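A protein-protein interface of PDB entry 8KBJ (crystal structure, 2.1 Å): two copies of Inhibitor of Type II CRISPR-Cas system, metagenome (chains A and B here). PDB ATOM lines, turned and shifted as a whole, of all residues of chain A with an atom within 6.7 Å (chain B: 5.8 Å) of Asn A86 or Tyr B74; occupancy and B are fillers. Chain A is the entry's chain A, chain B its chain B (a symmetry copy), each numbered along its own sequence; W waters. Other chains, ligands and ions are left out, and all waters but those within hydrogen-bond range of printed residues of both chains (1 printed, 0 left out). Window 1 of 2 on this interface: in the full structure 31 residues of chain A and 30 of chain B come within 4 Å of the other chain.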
ATOM      1  N   PHE A  30      -3.837   2.967  -6.186  1.00  0.00           N
ATOM      2  CA  PHE A  30      -2.439   2.635  -6.419  1.00  0.00           C
ATOM      3  C   PHE A  30      -2.258   2.410  -7.911  1.00  0.00           C
ATOM      4  O   PHE A  30      -3.222   2.228  -8.662  1.00  0.00           O
ATOM      5  CB  PHE A  30      -1.975   1.386  -5.623  1.00  0.00           C
ATOM      6  CG  PHE A  30      -2.776   0.145  -5.902  1.00  0.00           C
ATOM      7  CD1 PHE A  30      -3.972  -0.105  -5.227  1.00  0.00           C
ATOM      8  CD2 PHE A  30      -2.331  -0.789  -6.815  1.00  0.00           C
ATOM      9  CE1 PHE A  30      -4.710  -1.283  -5.481  1.00  0.00           C
ATOM     10  CE2 PHE A  30      -3.060  -1.968  -7.093  1.00  0.00           C
ATOM     11  CZ  PHE A  30      -4.234  -2.230  -6.439  1.00  0.00           C
ATOM     12  N   ARG A  32      -0.659   0.383 -11.249  1.00  0.00           N
ATOM     13  CA  ARG A  32      -0.109  -0.856 -11.736  1.00  0.00           C
ATOM     14  C   ARG A  32       0.695  -0.530 -12.975  1.00  0.00           C
ATOM     15  O   ARG A  32       0.240   0.280 -13.807  1.00  0.00           O
ATOM     16  CB  ARG A  32      -1.202  -1.892 -12.034  1.00  0.00           C
ATOM     17  CG  ARG A  32      -1.909  -2.312 -10.779  1.00  0.00           C
ATOM     18  CD  ARG A  32      -2.904  -3.489 -11.011  1.00  0.00           C
ATOM     19  NE  ARG A  32      -2.208  -4.765 -11.242  1.00  0.00           N
ATOM     20  CZ  ARG A  32      -2.822  -5.925 -11.440  1.00  0.00           C
ATOM     21  NH1 ARG A  32      -4.141  -6.010 -11.508  1.00  0.00           N
ATOM     22  NH2 ARG A  32      -2.099  -7.035 -11.519  1.00  0.00           N
ATOM     23  N   LYS A  47      -5.287 -14.889 -17.883  1.00  0.00           N
ATOM     24  CA  LYS A  47      -6.648 -15.091 -17.384  1.00  0.00           C
ATOM     25  C   LYS A  47      -7.545 -13.889 -17.652  1.00  0.00           C
ATOM     26  O   LYS A  47      -7.088 -12.751 -17.832  1.00  0.00           O
ATOM     27  CB  LYS A  47      -6.663 -15.255 -15.860  1.00  0.00           C
ATOM     28  CG  LYS A  47      -6.481 -16.638 -15.265  1.00  0.00           C
ATOM     29  CD  LYS A  47      -7.686 -16.976 -14.381  1.00  0.00           C
ATOM     30  CE  LYS A  47      -7.299 -17.570 -13.031  1.00  0.00           C
ATOM     31  NZ  LYS A  47      -8.391 -17.356 -12.032  1.00  0.00           N
ATOM     32  N   SER A  48      -8.851 -14.154 -17.606  1.00  0.00           N
ATOM     33  CA  SER A  48      -9.846 -13.092 -17.576  1.00  0.00           C
ATOM     34  C   SER A  48      -9.828 -12.281 -18.864  1.00  0.00           C
ATOM     35  O   SER A  48     -10.043 -11.070 -18.833  1.00  0.00           O
ATOM     36  CB  SER A  48      -9.639 -12.175 -16.364  1.00  0.00           C
ATOM     37  OG  SER A  48      -9.681 -12.944 -15.168  1.00  0.00           O
ATOM     38  N   TYR A  74      -1.874   1.774 -15.338  1.00  0.00           N
ATOM     39  CA  TYR A  74      -3.211   2.278 -15.019  1.00  0.00           C
ATOM     40  C   TYR A  74      -3.368   2.297 -13.506  1.00  0.00           C
ATOM     41  O   TYR A  74      -2.590   1.680 -12.787  1.00  0.00           O
ATOM     42  CB  TYR A  74      -4.305   1.409 -15.665  1.00  0.00           C
ATOM     43  CG  TYR A  74      -4.253  -0.071 -15.260  1.00  0.00           C
ATOM     44  CD1 TYR A  74      -3.312  -0.933 -15.826  1.00  0.00           C
ATOM     45  CD2 TYR A  74      -5.137  -0.585 -14.306  1.00  0.00           C
ATOM     46  CE1 TYR A  74      -3.267  -2.273 -15.482  1.00  0.00           C
ATOM     47  CE2 TYR A  74      -5.105  -1.901 -13.963  1.00  0.00           C
ATOM     48  CZ  TYR A  74      -4.173  -2.741 -14.558  1.00  0.00           C
ATOM     49  OH  TYR A  74      -4.130  -4.045 -14.232  1.00  0.00           O
ATOM     50  N   LEU A  75      -4.418   2.964 -13.043  1.00  0.00           N
ATOM     51  CA  LEU A  75      -4.745   3.119 -11.638  1.00  0.00           C
ATOM     52  C   LEU A  75      -5.836   2.137 -11.233  1.00  0.00           C
ATOM     53  O   LEU A  75      -6.739   1.807 -12.028  1.00  0.00           O
ATOM     54  CB  LEU A  75      -5.203   4.558 -11.319  1.00  0.00           C
ATOM     55  CG  LEU A  75      -4.114   5.619 -11.690  1.00  0.00           C
ATOM     56  CD1 LEU A  75      -4.521   7.115 -11.349  1.00  0.00           C
ATOM     57  CD2 LEU A  75      -2.725   5.224 -11.052  1.00  0.00           C
ATOM     58  N   CYS A  76      -5.739   1.757  -9.961  1.00  0.00           N
ATOM     59  CA  CYS A  76      -6.645   0.833  -9.369  1.00  0.00           C
ATOM     60  C   CYS A  76      -7.083   1.309  -8.005  1.00  0.00           C
ATOM     61  O   CYS A  76      -6.395   2.080  -7.398  1.00  0.00           O
ATOM     62  CB  CYS A  76      -5.925  -0.471  -9.172  1.00  0.00           C
ATOM     63  SG  CYS A  76      -5.501  -1.301 -10.682  1.00  0.00           S
ATOM     64  N   MET A  77      -8.207   0.818  -7.530  1.00  0.00           N
ATOM     65  CA  MET A  77      -8.697   1.156  -6.230  1.00  0.00           C
ATOM     66  C   MET A  77      -9.017   0.022  -5.286  1.00  0.00           C
ATOM     67  O   MET A  77      -9.599  -0.961  -5.725  1.00  0.00           O
ATOM     68  CB  MET A  77      -9.956   2.018  -6.375  1.00  0.00           C
ATOM     69  CG  MET A  77     -10.609   2.374  -5.051  1.00  0.00           C
ATOM     70  SD  MET A  77     -12.218   3.476  -5.235  1.00  0.00           S
ATOM     71  CE  MET A  77     -11.544   5.024  -4.238  1.00  0.00           C
ATOM     72  N   ILE A  84     -11.064  -5.022  -5.165  1.00  0.00           N
ATOM     73  CA  ILE A  84     -10.099  -4.274  -5.957  1.00  0.00           C
ATOM     74  C   ILE A  84     -10.742  -3.944  -7.282  1.00  0.00           C
ATOM     75  O   ILE A  84     -11.182  -4.847  -7.996  1.00  0.00           O
ATOM     76  CB  ILE A  84      -8.798  -5.054  -6.198  1.00  0.00           C
ATOM     77  CG1 ILE A  84      -8.226  -5.565  -4.887  1.00  0.00           C
ATOM     78  CG2 ILE A  84      -7.783  -4.117  -6.903  1.00  0.00           C
ATOM     79  CD1 ILE A  84      -7.785  -4.419  -3.971  1.00  0.00           C
ATOM     80  N   VAL A  85     -10.733  -2.677  -7.646  1.00  0.00           N
ATOM     81  CA  VAL A  85     -11.296  -2.213  -8.914  1.00  0.00           C
ATOM     82  C   VAL A  85     -10.120  -1.868  -9.818  1.00  0.00           C
ATOM     83  O   VAL A  85      -9.342  -0.957  -9.509  1.00  0.00           O
ATOM     84  CB  VAL A  85     -12.206  -1.000  -8.712  1.00  0.00           C
ATOM     85  CG1 VAL A  85     -12.721  -0.496 -10.065  1.00  0.00           C
ATOM     86  CG2 VAL A  85     -13.369  -1.342  -7.778  1.00  0.00           C
ATOM     87  N   ASN A  86      -9.945  -2.618 -10.900  1.00  0.00           N
ATOM     88  CA  ASN A  86      -8.961  -2.255 -11.910  1.00  0.00           C
ATOM     89  C   ASN A  86      -9.530  -1.102 -12.723  1.00  0.00           C
ATOM     90  O   ASN A  86     -10.669  -1.168 -13.194  1.00  0.00           O
ATOM     91  CB  ASN A  86      -8.623  -3.453 -12.823  1.00  0.00           C
ATOM     92  CG  ASN A  86      -7.716  -4.486 -12.129  1.00  0.00           C
ATOM     93  OD1 ASN A  86      -6.532  -4.251 -11.905  1.00  0.00           O
ATOM     94  ND2 ASN A  86      -8.275  -5.643 -11.824  1.00  0.00           N
ATOM     95  N   GLY A  87      -8.773  -0.025 -12.864  1.00  0.00           N
ATOM     96  CA  GLY A  87      -9.294   1.059 -13.697  1.00  0.00           C
ATOM     97  C   GLY A  87     -10.080   2.103 -12.922  1.00  0.00           C
ATOM     98  O   GLY A  87     -11.159   2.538 -13.363  1.00  0.00           O
ATOM     99  N   TRP A  88      -9.513   2.575 -11.812  1.00  0.00           N
ATOM    100  CA  TRP A  88     -10.139   3.640 -11.038  1.00  0.00           C
ATOM    101  C   TRP A  88     -10.265   4.907 -11.891  1.00  0.00           C
ATOM    102  O   TRP A  88      -9.373   5.231 -12.675  1.00  0.00           O
ATOM    103  CB  TRP A  88      -9.317   3.938  -9.773  1.00  0.00           C
ATOM    104  CG  TRP A  88      -9.751   5.255  -9.020  1.00  0.00           C
ATOM    105  CD1 TRP A  88     -10.771   5.386  -8.103  1.00  0.00           C
ATOM    106  CD2 TRP A  88      -9.142   6.539  -9.122  1.00  0.00           C
ATOM    107  NE1 TRP A  88     -10.833   6.707  -7.636  1.00  0.00           N
ATOM    108  CE2 TRP A  88      -9.844   7.424  -8.248  1.00  0.00           C
ATOM    109  CE3 TRP A  88      -8.058   7.032  -9.842  1.00  0.00           C
ATOM    110  CZ2 TRP A  88      -9.511   8.759  -8.124  1.00  0.00           C
ATOM    111  CZ3 TRP A  88      -7.716   8.374  -9.712  1.00  0.00           C
ATOM    112  CH2 TRP A  88      -8.433   9.222  -8.859  1.00  0.00           C
ATOM    113  N   PHE B  30     -13.791  -4.091 -24.527  1.00  0.00           N
ATOM    114  CA  PHE B  30     -14.193  -5.429 -24.127  1.00  0.00           C
ATOM    115  C   PHE B  30     -14.183  -5.498 -22.605  1.00  0.00           C
ATOM    116  O   PHE B  30     -13.549  -4.687 -21.934  1.00  0.00           O
ATOM    117  CB  PHE B  30     -13.311  -6.537 -24.761  1.00  0.00           C
ATOM    118  CG  PHE B  30     -11.848  -6.464 -24.396  1.00  0.00           C
ATOM    119  CD1 PHE B  30     -10.968  -5.684 -25.138  1.00  0.00           C
ATOM    120  CD2 PHE B  30     -11.350  -7.193 -23.315  1.00  0.00           C
ATOM    121  CE1 PHE B  30      -9.611  -5.586 -24.801  1.00  0.00           C
ATOM    122  CE2 PHE B  30      -9.983  -7.125 -22.974  1.00  0.00           C
ATOM    123  CZ  PHE B  30      -9.115  -6.323 -23.721  1.00  0.00           C
ATOM    124  N   MET B  31     -14.898  -6.479 -22.077  1.00  0.00           N
ATOM    125  CA  MET B  31     -15.043  -6.650 -20.637  1.00  0.00           C
ATOM    126  C   MET B  31     -14.139  -7.757 -20.067  1.00  0.00           C
ATOM    127  O   MET B  31     -14.037  -8.836 -20.645  1.00  0.00           O
ATOM    128  CB  MET B  31     -16.505  -6.979 -20.296  1.00  0.00           C
ATOM    129  CG  MET B  31     -16.691  -7.018 -18.792  1.00  0.00           C
ATOM    130  SD  MET B  31     -18.457  -7.495 -18.201  1.00  0.00           S
ATOM    131  CE  MET B  31     -18.036  -9.398 -18.038  1.00  0.00           C
ATOM    132  N   ARG B  32     -13.466  -7.493 -18.979  1.00  0.00           N
ATOM    133  CA  ARG B  32     -12.758  -8.583 -18.302  1.00  0.00           C
ATOM    134  C   ARG B  32     -13.545  -8.975 -17.046  1.00  0.00           C
ATOM    135  O   ARG B  32     -13.966  -8.097 -16.280  1.00  0.00           O
ATOM    136  CB  ARG B  32     -11.325  -8.184 -17.933  1.00  0.00           C
ATOM    137  CG  ARG B  32     -10.422  -7.864 -19.173  1.00  0.00           C
ATOM    138  CD  ARG B  32      -8.973  -7.516 -18.831  1.00  0.00           C
ATOM    139  NE  ARG B  32      -8.219  -8.696 -18.389  1.00  0.00           N
ATOM    140  CZ  ARG B  32      -6.913  -8.711 -18.181  1.00  0.00           C
ATOM    141  NH1 ARG B  32      -6.185  -7.618 -18.321  1.00  0.00           N
ATOM    142  NH2 ARG B  32      -6.319  -9.860 -17.832  1.00  0.00           N
ATOM    143  N   PRO B  33     -13.782 -10.267 -16.830  1.00  0.00           N
ATOM    144  CA  PRO B  33     -14.700 -10.700 -15.767  1.00  0.00           C
ATOM    145  C   PRO B  33     -14.071 -10.608 -14.382  1.00  0.00           C
ATOM    146  O   PRO B  33     -12.860 -10.560 -14.199  1.00  0.00           O
ATOM    147  CB  PRO B  33     -15.012 -12.175 -16.121  1.00  0.00           C
ATOM    148  CG  PRO B  33     -13.724 -12.642 -16.849  1.00  0.00           C
ATOM    149  CD  PRO B  33     -13.233 -11.393 -17.619  1.00  0.00           C
ATOM    150  N   GLU B  34     -14.948 -10.535 -13.398  1.00  0.00           N
ATOM    151  CA  GLU B  34     -14.516 -10.590 -12.017  1.00  0.00           C
ATOM    152  C   GLU B  34     -13.730 -11.869 -11.750  1.00  0.00           C
ATOM    153  O   GLU B  34     -13.866 -12.869 -12.455  1.00  0.00           O
ATOM    154  CB  GLU B  34     -15.714 -10.491 -11.098  1.00  0.00           C
ATOM    155  CG  GLU B  34     -16.378 -11.778 -10.827  1.00  0.00           C
ATOM    156  CD  GLU B  34     -17.198 -11.712  -9.558  1.00  0.00           C
ATOM    157  OE1 GLU B  34     -17.506 -10.574  -9.112  1.00  0.00           O
ATOM    158  OE2 GLU B  34     -17.504 -12.805  -9.004  1.00  0.00           O
ATOM    159  N   PHE B  71     -11.405  -9.168  -7.192  1.00  0.00           N
ATOM    160  CA  PHE B  71     -11.238  -8.139  -8.211  1.00  0.00           C
ATOM    161  C   PHE B  71     -12.505  -8.131  -9.046  1.00  0.00           C
ATOM    162  O   PHE B  71     -12.836  -9.143  -9.680  1.00  0.00           O
ATOM    163  CB  PHE B  71     -10.033  -8.429  -9.111  1.00  0.00           C
ATOM    164  CG  PHE B  71      -8.727  -8.554  -8.366  1.00  0.00           C
ATOM    165  CD1 PHE B  71      -8.490  -9.638  -7.509  1.00  0.00           C
ATOM    166  CD2 PHE B  71      -7.749  -7.574  -8.507  1.00  0.00           C
ATOM    167  CE1 PHE B  71      -7.297  -9.739  -6.799  1.00  0.00           C
ATOM    168  CE2 PHE B  71      -6.551  -7.654  -7.805  1.00  0.00           C
ATOM    169  CZ  PHE B  71      -6.318  -8.750  -6.947  1.00  0.00           C
ATOM    170  N   THR B  72     -13.194  -6.991  -9.073  1.00  0.00           N
ATOM    171  CA  THR B  72     -14.431  -6.887  -9.840  1.00  0.00           C
ATOM    172  C   THR B  72     -14.153  -6.844 -11.348  1.00  0.00           C
ATOM    173  O   THR B  72     -13.009  -6.706 -11.789  1.00  0.00           O
ATOM    174  CB  THR B  72     -15.219  -5.672  -9.380  1.00  0.00           C
ATOM    175  OG1 THR B  72     -14.408  -4.512  -9.517  1.00  0.00           O
ATOM    176  CG2 THR B  72     -15.551  -5.836  -7.910  1.00  0.00           C
ATOM    177  N   ALA B  73     -15.206  -7.092 -12.139  1.00  0.00           N
ATOM    178  CA  ALA B  73     -15.143  -6.962 -13.587  1.00  0.00           C
ATOM    179  C   ALA B  73     -14.869  -5.501 -14.002  1.00  0.00           C
ATOM    180  O   ALA B  73     -15.172  -4.559 -13.282  1.00  0.00           O
ATOM    181  CB  ALA B  73     -16.466  -7.446 -14.207  1.00  0.00           C
ATOM    182  N   TYR B  74     -14.331  -5.309 -15.201  1.00  0.00           N
ATOM    183  CA  TYR B  74     -14.068  -3.932 -15.635  1.00  0.00           C
ATOM    184  C   TYR B  74     -13.902  -3.919 -17.144  1.00  0.00           C
ATOM    185  O   TYR B  74     -13.691  -4.961 -17.755  1.00  0.00           O
ATOM    186  CB  TYR B  74     -12.812  -3.365 -14.935  1.00  0.00           C
ATOM    187  CG  TYR B  74     -11.559  -4.201 -15.159  1.00  0.00           C
ATOM    188  CD1 TYR B  74     -11.353  -5.401 -14.479  1.00  0.00           C
ATOM    189  CD2 TYR B  74     -10.608  -3.818 -16.104  1.00  0.00           C
ATOM    190  CE1 TYR B  74     -10.202  -6.177 -14.687  1.00  0.00           C
ATOM    191  CE2 TYR B  74      -9.458  -4.575 -16.323  1.00  0.00           C
ATOM    192  CZ  TYR B  74      -9.262  -5.748 -15.604  1.00  0.00           C
ATOM    193  OH  TYR B  74      -8.144  -6.485 -15.824  1.00  0.00           O
ATOM    194  N   LEU B  75     -13.941  -2.713 -17.744  1.00  0.00           N
ATOM    195  CA  LEU B  75     -13.811  -2.581 -19.182  1.00  0.00           C
ATOM    196  C   LEU B  75     -12.376  -2.196 -19.544  1.00  0.00           C
ATOM    197  O   LEU B  75     -11.672  -1.549 -18.761  1.00  0.00           O
ATOM    198  CB  LEU B  75     -14.820  -1.545 -19.733  1.00  0.00           C
ATOM    199  CG  LEU B  75     -16.282  -1.884 -19.366  1.00  0.00           C
ATOM    200  CD1 LEU B  75     -17.278  -0.807 -19.781  1.00  0.00           C
ATOM    201  CD2 LEU B  75     -16.708  -3.287 -19.946  1.00  0.00           C
ATOM    202  N   CYS B  76     -11.949  -2.639 -20.735  1.00  0.00           N
ATOM    203  CA  CYS B  76     -10.627  -2.440 -21.316  1.00  0.00           C
ATOM    204  C   CYS B  76     -10.791  -1.993 -22.758  1.00  0.00           C
ATOM    205  O   CYS B  76     -11.810  -2.252 -23.393  1.00  0.00           O
ATOM    206  CB  CYS B  76      -9.779  -3.720 -21.320  1.00  0.00           C
ATOM    207  SG  CYS B  76      -9.630  -4.337 -19.702  1.00  0.00           S
ATOM    208  N   ASN B  86      -6.189  -1.259 -19.587  1.00  0.00           N
ATOM    209  CA  ASN B  86      -7.073  -1.751 -18.539  1.00  0.00           C
ATOM    210  C   ASN B  86      -7.763  -0.538 -17.906  1.00  0.00           C
ATOM    211  O   ASN B  86      -7.113   0.433 -17.544  1.00  0.00           O
ATOM    212  CB  ASN B  86      -6.303  -2.515 -17.462  1.00  0.00           C
ATOM    213  CG  ASN B  86      -5.843  -3.894 -17.931  1.00  0.00           C
ATOM    214  OD1 ASN B  86      -6.647  -4.820 -18.103  1.00  0.00           O
ATOM    215  ND2 ASN B  86      -4.549  -4.043 -18.101  1.00  0.00           N
ATOM    216  N   GLY B  87      -9.073  -0.578 -17.807  1.00  0.00           N
ATOM    217  CA  GLY B  87      -9.800   0.477 -17.126  1.00  0.00           C
ATOM    218  C   GLY B  87     -10.263   1.579 -18.045  1.00  0.00           C
ATOM    219  O   GLY B  87     -10.100   2.762 -17.729  1.00  0.00           O
HETATM  220  O   HOH W   1     -10.816  -5.271 -10.770  1.00  0.00           O
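Asn A86 touches two residues of chain B. Of chain A, only Asn A86 (3.5 Å) comes within 4 Å of Tyr B74. Printed residues of chain A within 4 Å of Phe B71: Ile A84 (3.3 Å) and Asn A86 (3.9 Å). Of the printed residues of chain A, Asn B86 touches Tyr A74. Of the printed residues of chain A, Pro B33 touches Ser A48 (3.4 Å). Leu B75 touches none of the printed residues of chain A. Cys B76 touches none of the printed residues of chain A. The nearest residue of chain B that does not touch Asn A86 is Gly B87 (4.3 Å).
The backbone NH (N) of Arg A32 is in hydrogen-bond range of the backbone carbonyl oxygen (O) of Tyr A74 (2.8 Å). OH of Tyr A74 sits at hydrogen-bond distance from OD1 of Asn A86 (3.4 Å). The backbone NH (N) of Gly A87 is in hydrogen-bond range of the backbone carbonyl oxygen (O) of Leu A75 (2.9 Å). The side-chain amide oxygen (OD1) of Asn B86 lies within hydrogen-bond range of the side-chain hydroxyl (OH) of Tyr B74 (3.2 Å). The backbone carbonyl oxygen (O) of Leu B75 lies within hydrogen-bond range of the backbone NH (N) of Gly B87 (2.9 Å). The side-chain sulfur (SG) of Cys B76 sits at hydrogen-bond distance from the side-chain amide oxygen (OD1) of Asn B86 (3.4 Å).
CD of Pro B33 touches O of Ser A48 (3.4 Å). Tyr A74 touches Asn B86. CA of Phe B71 touches O of Ile A84, at 3.3 Å. Val A85 touches Thr B72 (CG2 to OG1, 3.8 Å). Phe B71 touches Asn A86 (CD2 to ND2, 3.9 Å). Asn A86 touches Tyr B74. CA of Gly A87 touches CA of Gly B87, 3.5 Å away.
Water W1 lies within hydrogen-bond range of ND2 of Asn A86, O of Thr B72 and O of Ile A84.
Tyr A74 touches Asn B86, and with the chains exchanged Asn A86 touches Tyr B74. Gly A87 touches its own counterpart, Gly B87. Positions printed for both chains: 30, 32, 74, 75, 76, 86 and 87. Of the 10 pairs that touch across the chains among the printed residues, 3 have their exchanged pair printed and touching as well.
NH2 of Arg B32 lies within hydrogen-bond range of O of Lys A47, 3.0 Å away. The backbone carbonyl oxygen of Ser A48 sits at hydrogen-bond distance from the guanidinium group of Arg B32 (3.0 Å). N of Thr B72 is in hydrogen-bond range of O of Ile A84 (3.1 Å).
Of the 13 printed residues of chain A, 7 touch a printed residue of chain B. Along chain A the printed residues that touch a printed residue of chain B span positions 47 to 87. Of the 13 printed residues of chain B, 7 touch a printed residue of chain A. Printed residues of chain B that touch a printed residue of chain A: Arg B32, Pro B33, Phe B71, Thr B72, Tyr B74, Asn B86 and Gly B87.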
